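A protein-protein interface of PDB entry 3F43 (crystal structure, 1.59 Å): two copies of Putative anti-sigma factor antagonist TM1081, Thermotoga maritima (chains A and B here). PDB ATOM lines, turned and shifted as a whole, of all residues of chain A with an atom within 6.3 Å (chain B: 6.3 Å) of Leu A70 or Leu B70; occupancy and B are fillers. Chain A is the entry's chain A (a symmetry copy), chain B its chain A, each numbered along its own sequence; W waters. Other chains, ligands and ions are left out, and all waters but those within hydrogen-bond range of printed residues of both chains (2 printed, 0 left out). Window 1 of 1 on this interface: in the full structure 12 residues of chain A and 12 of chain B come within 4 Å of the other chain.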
ATOM      1  N   ILE A  65       5.238 -34.417 -22.929  1.00  0.00           N
ATOM      2  CA  ILE A  65       5.932 -33.953 -21.735  1.00  0.00           C
ATOM      3  C   ILE A  65       5.585 -32.496 -21.495  1.00  0.00           C
ATOM      4  O   ILE A  65       5.233 -31.755 -22.423  1.00  0.00           O
ATOM      5  CB  ILE A  65       7.469 -34.112 -21.799  1.00  0.00           C
ATOM      6  CG1 ILE A  65       8.016 -33.432 -23.053  1.00  0.00           C
ATOM      7  CG2 ILE A  65       7.878 -35.648 -21.705  1.00  0.00           C
ATOM      8  CD1 ILE A  65       9.575 -33.285 -23.094  1.00  0.00           C
ATOM      9  N   ASP A  66       5.689 -32.109 -20.238  1.00  0.00           N
ATOM     10  CA  ASP A  66       5.416 -30.746 -19.794  1.00  0.00           C
ATOM     11  C   ASP A  66       6.650 -30.164 -19.122  1.00  0.00           C
ATOM     12  O   ASP A  66       7.732 -30.801 -19.104  1.00  0.00           O
ATOM     13  CB  ASP A  66       4.103 -30.682 -18.966  1.00  0.00           C
ATOM     14  CG  ASP A  66       4.202 -31.273 -17.532  1.00  0.00           C
ATOM     15  OD1 ASP A  66       5.318 -31.553 -17.057  1.00  0.00           O
ATOM     16  OD2 ASP A  66       3.091 -31.401 -16.903  1.00  0.00           O
ATOM     17  N   SER A  67       6.527 -28.958 -18.553  1.00  0.00           N
ATOM     18  CA  SER A  67       7.686 -28.284 -17.989  1.00  0.00           C
ATOM     19  C   SER A  67       8.255 -29.046 -16.805  1.00  0.00           C
ATOM     20  O   SER A  67       9.465 -29.025 -16.572  1.00  0.00           O
ATOM     21  CB  SER A  67       7.351 -26.847 -17.592  1.00  0.00           C
ATOM     22  OG  SER A  67       6.421 -26.789 -16.526  1.00  0.00           O
ATOM     23  N   PHE A  68       7.384 -29.724 -16.056  1.00  0.00           N
ATOM     24  CA  PHE A  68       7.826 -30.523 -14.918  1.00  0.00           C
ATOM     25  C   PHE A  68       8.559 -31.762 -15.329  1.00  0.00           C
ATOM     26  O   PHE A  68       9.628 -32.066 -14.752  1.00  0.00           O
ATOM     27  CB  PHE A  68       6.638 -30.866 -13.978  1.00  0.00           C
ATOM     28  CG  PHE A  68       6.284 -29.768 -13.031  1.00  0.00           C
ATOM     29  CD1 PHE A  68       5.810 -28.553 -13.493  1.00  0.00           C
ATOM     30  CD2 PHE A  68       6.403 -29.958 -11.673  1.00  0.00           C
ATOM     31  CE1 PHE A  68       5.512 -27.537 -12.613  1.00  0.00           C
ATOM     32  CE2 PHE A  68       6.067 -28.960 -10.790  1.00  0.00           C
ATOM     33  CZ  PHE A  68       5.627 -27.743 -11.251  1.00  0.00           C
ATOM     34  N   SER A  69       8.099 -32.454 -16.359  1.00  0.00           N
ATOM     35  CA  SER A  69       8.855 -33.642 -16.803  1.00  0.00           C
ATOM     36  C   SER A  69      10.176 -33.196 -17.459  1.00  0.00           C
ATOM     37  O   SER A  69      11.224 -33.856 -17.312  1.00  0.00           O
ATOM     38  CB  SER A  69       8.033 -34.622 -17.652  1.00  0.00           C
ATOM     39  OG  SER A  69       7.016 -34.030 -18.450  1.00  0.00           O
ATOM     40  N   LEU A  70      10.179 -32.036 -18.101  1.00  0.00           N
ATOM     41  CA  LEU A  70      11.437 -31.500 -18.613  1.00  0.00           C
ATOM     42  C   LEU A  70      12.401 -31.189 -17.475  1.00  0.00           C
ATOM     43  O   LEU A  70      13.603 -31.456 -17.568  1.00  0.00           O
ATOM     44  CB  LEU A  70      11.249 -30.217 -19.416  1.00  0.00           C
ATOM     45  CG  LEU A  70      10.972 -30.355 -20.882  1.00  0.00           C
ATOM     46  CD1 LEU A  70      10.633 -28.950 -21.453  1.00  0.00           C
ATOM     47  CD2 LEU A  70      12.183 -31.007 -21.599  1.00  0.00           C
ATOM     48  N   GLY A  71      11.907 -30.612 -16.382  1.00  0.00           N
ATOM     49  CA  GLY A  71      12.757 -30.326 -15.242  1.00  0.00           C
ATOM     50  C   GLY A  71      13.400 -31.588 -14.675  1.00  0.00           C
ATOM     51  O   GLY A  71      14.583 -31.589 -14.301  1.00  0.00           O
ATOM     52  N   VAL A  72      12.645 -32.676 -14.656  1.00  0.00           N
ATOM     53  CA  VAL A  72      13.179 -33.977 -14.227  1.00  0.00           C
ATOM     54  C   VAL A  72      14.286 -34.471 -15.168  1.00  0.00           C
ATOM     55  O   VAL A  72      15.370 -34.888 -14.718  1.00  0.00           O
ATOM     56  CB  VAL A  72      12.089 -34.982 -13.971  1.00  0.00           C
ATOM     57  CG1 VAL A  72      12.695 -36.393 -13.771  1.00  0.00           C
ATOM     58  CG2 VAL A  72      11.260 -34.467 -12.732  1.00  0.00           C
ATOM     59  N   ILE A  73      14.042 -34.387 -16.477  1.00  0.00           N
ATOM     60  CA  ILE A  73      15.050 -34.744 -17.461  1.00  0.00           C
ATOM     61  C   ILE A  73      16.335 -33.932 -17.262  1.00  0.00           C
ATOM     62  O   ILE A  73      17.453 -34.476 -17.255  1.00  0.00           O
ATOM     63  CB  ILE A  73      14.505 -34.597 -18.874  1.00  0.00           C
ATOM     64  CG1 ILE A  73      13.425 -35.666 -19.088  1.00  0.00           C
ATOM     65  CG2 ILE A  73      15.612 -34.692 -19.923  1.00  0.00           C
ATOM     66  CD1 ILE A  73      12.665 -35.500 -20.401  1.00  0.00           C
ATOM     67  N   VAL A  74      16.166 -32.633 -17.043  1.00  0.00           N
ATOM     68  CA  VAL A  74      17.284 -31.754 -16.787  1.00  0.00           C
ATOM     69  C   VAL A  74      18.029 -32.153 -15.525  1.00  0.00           C
ATOM     70  O   VAL A  74      19.247 -32.145 -15.513  1.00  0.00           O
ATOM     71  CB  VAL A  74      16.841 -30.271 -16.786  1.00  0.00           C
ATOM     72  CG1 VAL A  74      17.926 -29.350 -16.168  1.00  0.00           C
ATOM     73  CG2 VAL A  74      16.460 -29.840 -18.196  1.00  0.00           C
ATOM     74  N   ASN A  75      17.289 -32.498 -14.462  1.00  0.00           N
ATOM     75  CA  ASN A  75      17.948 -32.886 -13.226  1.00  0.00           C
ATOM     76  C   ASN A  75      18.764 -34.158 -13.398  1.00  0.00           C
ATOM     77  O   ASN A  75      19.873 -34.285 -12.863  1.00  0.00           O
ATOM     78  CB  ASN A  75      16.926 -33.074 -12.116  1.00  0.00           C
ATOM     79  CG  ASN A  75      16.470 -31.765 -11.526  1.00  0.00           C
ATOM     80  OD1 ASN A  75      17.234 -30.812 -11.432  1.00  0.00           O
ATOM     81  ND2 ASN A  75      15.217 -31.733 -11.106  1.00  0.00           N
ATOM     82  N   VAL A  99       9.025 -30.606 -28.489  1.00  0.00           N
ATOM     83  CA  VAL A  99       9.410 -29.913 -27.260  1.00  0.00           C
ATOM     84  C   VAL A  99      10.930 -29.996 -27.084  1.00  0.00           C
ATOM     85  O   VAL A  99      11.558 -28.994 -26.722  1.00  0.00           O
ATOM     86  CB  VAL A  99       8.646 -30.428 -26.033  1.00  0.00           C
ATOM     87  CG1 VAL A  99       9.314 -29.951 -24.711  1.00  0.00           C
ATOM     88  CG2 VAL A  99       7.167 -30.016 -26.142  1.00  0.00           C
ATOM     89  N   LEU A 100      11.515 -31.179 -27.335  1.00  0.00           N
ATOM     90  CA  LEU A 100      12.973 -31.388 -27.160  1.00  0.00           C
ATOM     91  C   LEU A 100      13.763 -30.473 -28.091  1.00  0.00           C
ATOM     92  O   LEU A 100      14.808 -29.969 -27.732  1.00  0.00           O
ATOM     93  CB  LEU A 100      13.349 -32.860 -27.392  1.00  0.00           C
ATOM     94  CG  LEU A 100      12.799 -33.894 -26.408  1.00  0.00           C
ATOM     95  CD1 LEU A 100      13.181 -35.338 -26.857  1.00  0.00           C
ATOM     96  CD2 LEU A 100      13.240 -33.635 -24.957  1.00  0.00           C
ATOM     97  N   THR A 103      13.201 -26.506 -27.104  1.00  0.00           N
ATOM     98  CA  THR A 103      13.919 -26.154 -25.881  1.00  0.00           C
ATOM     99  C   THR A 103      15.422 -26.446 -25.969  1.00  0.00           C
ATOM    100  O   THR A 103      16.124 -26.327 -24.987  1.00  0.00           O
ATOM    101  CB  THR A 103      13.355 -26.930 -24.674  1.00  0.00           C
ATOM    102  OG1 THR A 103      13.614 -28.341 -24.844  1.00  0.00           O
ATOM    103  CG2 THR A 103      11.847 -26.709 -24.517  1.00  0.00           C
ATOM    104  N   LEU A 105      17.051 -29.080 -26.076  1.00  0.00           N
ATOM    105  CA  LEU A 105      17.543 -30.221 -25.346  1.00  0.00           C
ATOM    106  C   LEU A 105      18.228 -31.214 -26.300  1.00  0.00           C
ATOM    107  O   LEU A 105      19.201 -31.863 -25.939  1.00  0.00           O
ATOM    108  CB  LEU A 105      16.409 -30.852 -24.545  1.00  0.00           C
ATOM    109  CG  LEU A 105      16.639 -31.758 -23.381  1.00  0.00           C
ATOM    110  CD1 LEU A 105      17.876 -31.503 -22.557  1.00  0.00           C
ATOM    111  CD2 LEU A 105      15.296 -31.719 -22.563  1.00  0.00           C
ATOM    112  N   ILE B  65      14.136 -19.240 -24.417  1.00  0.00           N
ATOM    113  CA  ILE B  65      14.432 -20.052 -23.245  1.00  0.00           C
ATOM    114  C   ILE B  65      14.696 -21.479 -23.686  1.00  0.00           C
ATOM    115  O   ILE B  65      14.220 -21.929 -24.737  1.00  0.00           O
ATOM    116  CB  ILE B  65      13.317 -20.041 -22.174  1.00  0.00           C
ATOM    117  CG1 ILE B  65      11.983 -20.444 -22.801  1.00  0.00           C
ATOM    118  CG2 ILE B  65      13.251 -18.626 -21.447  1.00  0.00           C
ATOM    119  CD1 ILE B  65      10.837 -20.736 -21.774  1.00  0.00           C
ATOM    120  N   ASP B  66      15.461 -22.173 -22.864  1.00  0.00           N
ATOM    121  CA  ASP B  66      15.824 -23.567 -23.093  1.00  0.00           C
ATOM    122  C   ASP B  66      15.362 -24.421 -21.921  1.00  0.00           C
ATOM    123  O   ASP B  66      14.674 -23.923 -20.996  1.00  0.00           O
ATOM    124  CB  ASP B  66      17.326 -23.698 -23.471  1.00  0.00           C
ATOM    125  CG  ASP B  66      18.319 -23.491 -22.294  1.00  0.00           C
ATOM    126  OD1 ASP B  66      17.891 -23.453 -21.126  1.00  0.00           O
ATOM    127  OD2 ASP B  66      19.558 -23.409 -22.617  1.00  0.00           O
ATOM    128  N   SER B  67      15.722 -25.710 -21.923  1.00  0.00           N
ATOM    129  CA  SER B  67      15.227 -26.618 -20.900  1.00  0.00           C
ATOM    130  C   SER B  67      15.731 -26.234 -19.520  1.00  0.00           C
ATOM    131  O   SER B  67      15.037 -26.436 -18.523  1.00  0.00           O
ATOM    132  CB  SER B  67      15.594 -28.066 -21.221  1.00  0.00           C
ATOM    133  OG  SER B  67      16.992 -28.289 -21.171  1.00  0.00           O
ATOM    134  N   PHE B  68      16.941 -25.675 -19.460  1.00  0.00           N
ATOM    135  CA  PHE B  68      17.507 -25.231 -18.190  1.00  0.00           C
ATOM    136  C   PHE B  68      16.828 -24.011 -17.648  1.00  0.00           C
ATOM    137  O   PHE B  68      16.508 -23.970 -16.439  1.00  0.00           O
ATOM    138  CB  PHE B  68      19.040 -25.009 -18.306  1.00  0.00           C
ATOM    139  CG  PHE B  68      19.840 -26.264 -18.188  1.00  0.00           C
ATOM    140  CD1 PHE B  68      19.727 -27.273 -19.128  1.00  0.00           C
ATOM    141  CD2 PHE B  68      20.725 -26.427 -17.147  1.00  0.00           C
ATOM    142  CE1 PHE B  68      20.449 -28.438 -18.996  1.00  0.00           C
ATOM    143  CE2 PHE B  68      21.477 -27.571 -17.034  1.00  0.00           C
ATOM    144  CZ  PHE B  68      21.340 -28.586 -17.951  1.00  0.00           C
ATOM    145  N   SER B  69      16.505 -23.043 -18.491  1.00  0.00           N
ATOM    146  CA  SER B  69      15.782 -21.866 -17.968  1.00  0.00           C
ATOM    147  C   SER B  69      14.343 -22.271 -17.594  1.00  0.00           C
ATOM    148  O   SER B  69      13.772 -21.779 -16.600  1.00  0.00           O
ATOM    149  CB  SER B  69      15.870 -20.629 -18.871  1.00  0.00           C
ATOM    150  OG  SER B  69      15.971 -20.898 -20.263  1.00  0.00           O
ATOM    151  N   LEU B  70      13.773 -23.232 -18.308  1.00  0.00           N
ATOM    152  CA  LEU B  70      12.469 -23.751 -17.904  1.00  0.00           C
ATOM    153  C   LEU B  70      12.552 -24.430 -16.542  1.00  0.00           C
ATOM    154  O   LEU B  70      11.663 -24.274 -15.698  1.00  0.00           O
ATOM    155  CB  LEU B  70      11.908 -24.771 -18.890  1.00  0.00           C
ATOM    156  CG  LEU B  70      11.094 -24.249 -20.034  1.00  0.00           C
ATOM    157  CD1 LEU B  70      10.789 -25.428 -21.000  1.00  0.00           C
ATOM    158  CD2 LEU B  70       9.803 -23.569 -19.507  1.00  0.00           C
ATOM    159  N   GLY B  71      13.606 -25.205 -16.297  1.00  0.00           N
ATOM    160  CA  GLY B  71      13.772 -25.849 -15.007  1.00  0.00           C
ATOM    161  C   GLY B  71      13.844 -24.838 -13.866  1.00  0.00           C
ATOM    162  O   GLY B  71      13.269 -25.051 -12.788  1.00  0.00           O
ATOM    163  N   VAL B  72      14.504 -23.716 -14.114  1.00  0.00           N
ATOM    164  CA  VAL B  72      14.560 -22.623 -13.133  1.00  0.00           C
ATOM    165  C   VAL B  72      13.170 -22.030 -12.868  1.00  0.00           C
ATOM    166  O   VAL B  72      12.760 -21.850 -11.706  1.00  0.00           O
ATOM    167  CB  VAL B  72      15.613 -21.605 -13.476  1.00  0.00           C
ATOM    168  CG1 VAL B  72      15.470 -20.357 -12.570  1.00  0.00           C
ATOM    169  CG2 VAL B  72      17.014 -22.321 -13.351  1.00  0.00           C
ATOM    170  N   ILE B  73      12.417 -21.763 -13.938  1.00  0.00           N
ATOM    171  CA  ILE B  73      11.054 -21.280 -13.806  1.00  0.00           C
ATOM    172  C   ILE B  73      10.200 -22.245 -12.973  1.00  0.00           C
ATOM    173  O   ILE B  73       9.471 -21.837 -12.053  1.00  0.00           O
ATOM    174  CB  ILE B  73      10.435 -21.018 -15.171  1.00  0.00           C
ATOM    175  CG1 ILE B  73      11.160 -19.824 -15.807  1.00  0.00           C
ATOM    176  CG2 ILE B  73       8.929 -20.783 -15.077  1.00  0.00           C
ATOM    177  CD1 ILE B  73      10.762 -19.583 -17.260  1.00  0.00           C
ATOM    178  N   VAL B  74      10.339 -23.533 -13.264  1.00  0.00           N
ATOM    179  CA  VAL B  74       9.637 -24.558 -12.526  1.00  0.00           C
ATOM    180  C   VAL B  74      10.033 -24.561 -11.060  1.00  0.00           C
ATOM    181  O   VAL B  74       9.180 -24.697 -10.203  1.00  0.00           O
ATOM    182  CB  VAL B  74       9.798 -25.942 -13.202  1.00  0.00           C
ATOM    183  CG1 VAL B  74       9.368 -27.093 -12.253  1.00  0.00           C
ATOM    184  CG2 VAL B  74       9.037 -25.972 -14.520  1.00  0.00           C
ATOM    185  N   ASN B  75      11.336 -24.414 -10.780  1.00  0.00           N
ATOM    186  CA  ASN B  75      11.775 -24.412  -9.394  1.00  0.00           C
ATOM    187  C   ASN B  75      11.208 -23.228  -8.626  1.00  0.00           C
ATOM    188  O   ASN B  75      10.810 -23.351  -7.460  1.00  0.00           O
ATOM    189  CB  ASN B  75      13.293 -24.399  -9.318  1.00  0.00           C
ATOM    190  CG  ASN B  75      13.893 -25.758  -9.563  1.00  0.00           C
ATOM    191  OD1 ASN B  75      13.321 -26.779  -9.200  1.00  0.00           O
ATOM    192  ND2 ASN B  75      15.070 -25.763 -10.165  1.00  0.00           N
ATOM    193  N   VAL B  99       7.176 -21.933 -26.438  1.00  0.00           N
ATOM    194  CA  VAL B  99       7.692 -22.944 -25.515  1.00  0.00           C
ATOM    195  C   VAL B  99       6.748 -23.064 -24.313  1.00  0.00           C
ATOM    196  O   VAL B  99       6.455 -24.183 -23.878  1.00  0.00           O
ATOM    197  CB  VAL B  99       9.144 -22.671 -25.099  1.00  0.00           C
ATOM    198  CG1 VAL B  99       9.546 -23.525 -23.862  1.00  0.00           C
ATOM    199  CG2 VAL B  99      10.071 -22.889 -26.308  1.00  0.00           C
ATOM    200  N   LEU B 100       6.282 -21.922 -23.781  1.00  0.00           N
ATOM    201  CA  LEU B 100       5.394 -21.914 -22.593  1.00  0.00           C
ATOM    202  C   LEU B 100       4.090 -22.648 -22.890  1.00  0.00           C
ATOM    203  O   LEU B 100       3.550 -23.330 -22.043  1.00  0.00           O
ATOM    204  CB  LEU B 100       5.118 -20.477 -22.123  1.00  0.00           C
ATOM    205  CG  LEU B 100       6.301 -19.666 -21.593  1.00  0.00           C
ATOM    206  CD1 LEU B 100       5.866 -18.203 -21.272  1.00  0.00           C
ATOM    207  CD2 LEU B 100       6.977 -20.318 -20.375  1.00  0.00           C
ATOM    208  N   THR B 103       4.769 -26.656 -23.598  1.00  0.00           N
ATOM    209  CA  THR B 103       5.081 -27.370 -22.361  1.00  0.00           C
ATOM    210  C   THR B 103       3.986 -27.222 -21.297  1.00  0.00           C
ATOM    211  O   THR B 103       4.164 -27.651 -20.176  1.00  0.00           O
ATOM    212  CB  THR B 103       6.403 -26.862 -21.755  1.00  0.00           C
ATOM    213  OG1 THR B 103       6.246 -25.487 -21.340  1.00  0.00           O
ATOM    214  CG2 THR B 103       7.557 -26.958 -22.758  1.00  0.00           C
ATOM    215  N   LEU B 105       3.030 -24.825 -19.581  1.00  0.00           N
ATOM    216  CA  LEU B 105       3.310 -23.955 -18.467  1.00  0.00           C
ATOM    217  C   LEU B 105       2.261 -22.835 -18.383  1.00  0.00           C
ATOM    218  O   LEU B 105       1.891 -22.398 -17.301  1.00  0.00           O
ATOM    219  CB  LEU B 105       4.737 -23.428 -18.567  1.00  0.00           C
ATOM    220  CG  LEU B 105       5.482 -22.865 -17.402  1.00  0.00           C
ATOM    221  CD1 LEU B 105       5.157 -23.441 -16.047  1.00  0.00           C
ATOM    222  CD2 LEU B 105       7.000 -22.966 -17.802  1.00  0.00           C
HETATM  223  O   HOH W   1       3.931 -27.160 -17.484  1.00  0.00           O
HETATM  224  O   HOH W   2      18.121 -27.438 -23.464  1.00  0.00           O
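The backbone NH (N) of Asp B66 lies within hydrogen-bond range of the side-chain hydroxyl (OG) of Ser B69 (2.9 Å).
The backbone carbonyl oxygen (O) of Val B99 sits at hydrogen-bond distance from the side-chain hydroxyl (OG1) of Thr B103 (2.9 Å).
The backbone carbonyl oxygen (O) of Leu B100 is in hydrogen-bond range of the backbone NH (N) of Leu B105 (2.9 Å).
The side-chain carboxylate (OD1) of Asp A66 lies within hydrogen-bond range of the backbone NH (N) of Phe A68.
OG of Ser A69 lies within hydrogen-bond range of N of Asp A66, 2.9 Å away.
The side-chain hydroxyl (OG1) of Thr A103 is in hydrogen-bond range of the backbone carbonyl oxygen (O) of Val A99, 2.9 Å away.
Hydrophobic or aromatic side chains of chain A within 4 Å of the printed part of chain B: Phe A68, Leu A70, Val A74, Val A99 and Leu A105.
Hydrophobic or aromatic side chains of chain B that line the printed part of chain A: Phe B68, Leu B70, Val B74, Val B99 and Leu B105.
Along chain B the printed residues that touch a printed residue of chain A span positions 66 to 105.
Among the printed residues, no Asp or Glu carboxylate lies within 4 Å of a Lys or Arg side-chain nitrogen of the other chain.
Leu A70 touches just these residues of chain B: Leu B70 and Thr B103.
Printed residues of chain A within 4 Å of Leu B70: Leu A70 and Thr A103.
Of the printed residues of chain A, Val B99 touches Thr A103 (3.98 Å).
Printed residues of chain A within 4 Å of Ser B67: Val A74, Thr A103 and Leu A105.
Printed residues of chain A within 4 Å of Val B74: Ser A67 (3.4 Å) and Phe A68 (3.9 Å).
Leu B100 touches none of the printed residues of chain A.
Gly B71 touches none of the printed residues of chain A.
The nearest residue of chain B that does not touch Leu A70 is Ser B67 (4.5 Å).
Asp A66 touches Thr B103 (CB to O, 3.3 Å).
OG of Ser A67 touches CG2 of Val B74 (3.4 Å).
Val B74 touches Phe A68 (CG1 to CE1, 3.9 Å).
Leu B70 touches Leu A70 (CD1 to CD1, 3.6 Å).
CD1 of Leu A70 touches CG2 of Thr B103, 3.9 Å away.
Val A74 touches Phe B68 (CG1 to CE1, 3.9 Å).
CG2 of Thr B103 touches CG1 of Val A99 (3.98 Å).
O of Thr A103 touches CB of Asp B66, 3.3 Å away.
CG2 of Thr A103 touches CG1 of Val B99, at 3.98 Å.
Leu A105 touches Ser B67 (CD1 to OG, 3.6 Å).
Water W2 lies within hydrogen-bond range of OG of Ser B67 (2.7 Å), O of Thr A103 (2.7 Å) and N of Leu A105 (3.3 Å).
Water W1 lies within hydrogen-bond range of OG of Ser A67, O of Thr B103 and N of Leu B105.
The backbone carbonyl oxygen (O) of Thr A103 lies within hydrogen-bond range of the backbone NH (N) of Ser B67 (3.2 Å).
O of Thr B103 sits at hydrogen-bond distance from N of Ser A67.
Ser A67 touches Leu B105, and with the chains exchanged Leu A105 touches Ser B67.
Phe A68 touches Val B74, and with the chains exchanged Val A74 touches Phe B68.
Leu A70 touches its own counterpart, Leu B70.
Leu A70 touches Thr B103, and with the chains exchanged Thr A103 touches Leu B70.
Positions printed for both chains: 65, 66, 67, 68, 69, 70, 71, 72, 73, 74, 75, 99, 100, 103 and 105.
Of the 15 pairs that touch across the chains among the printed residues, 15 have their exchanged pair printed and touching as well.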
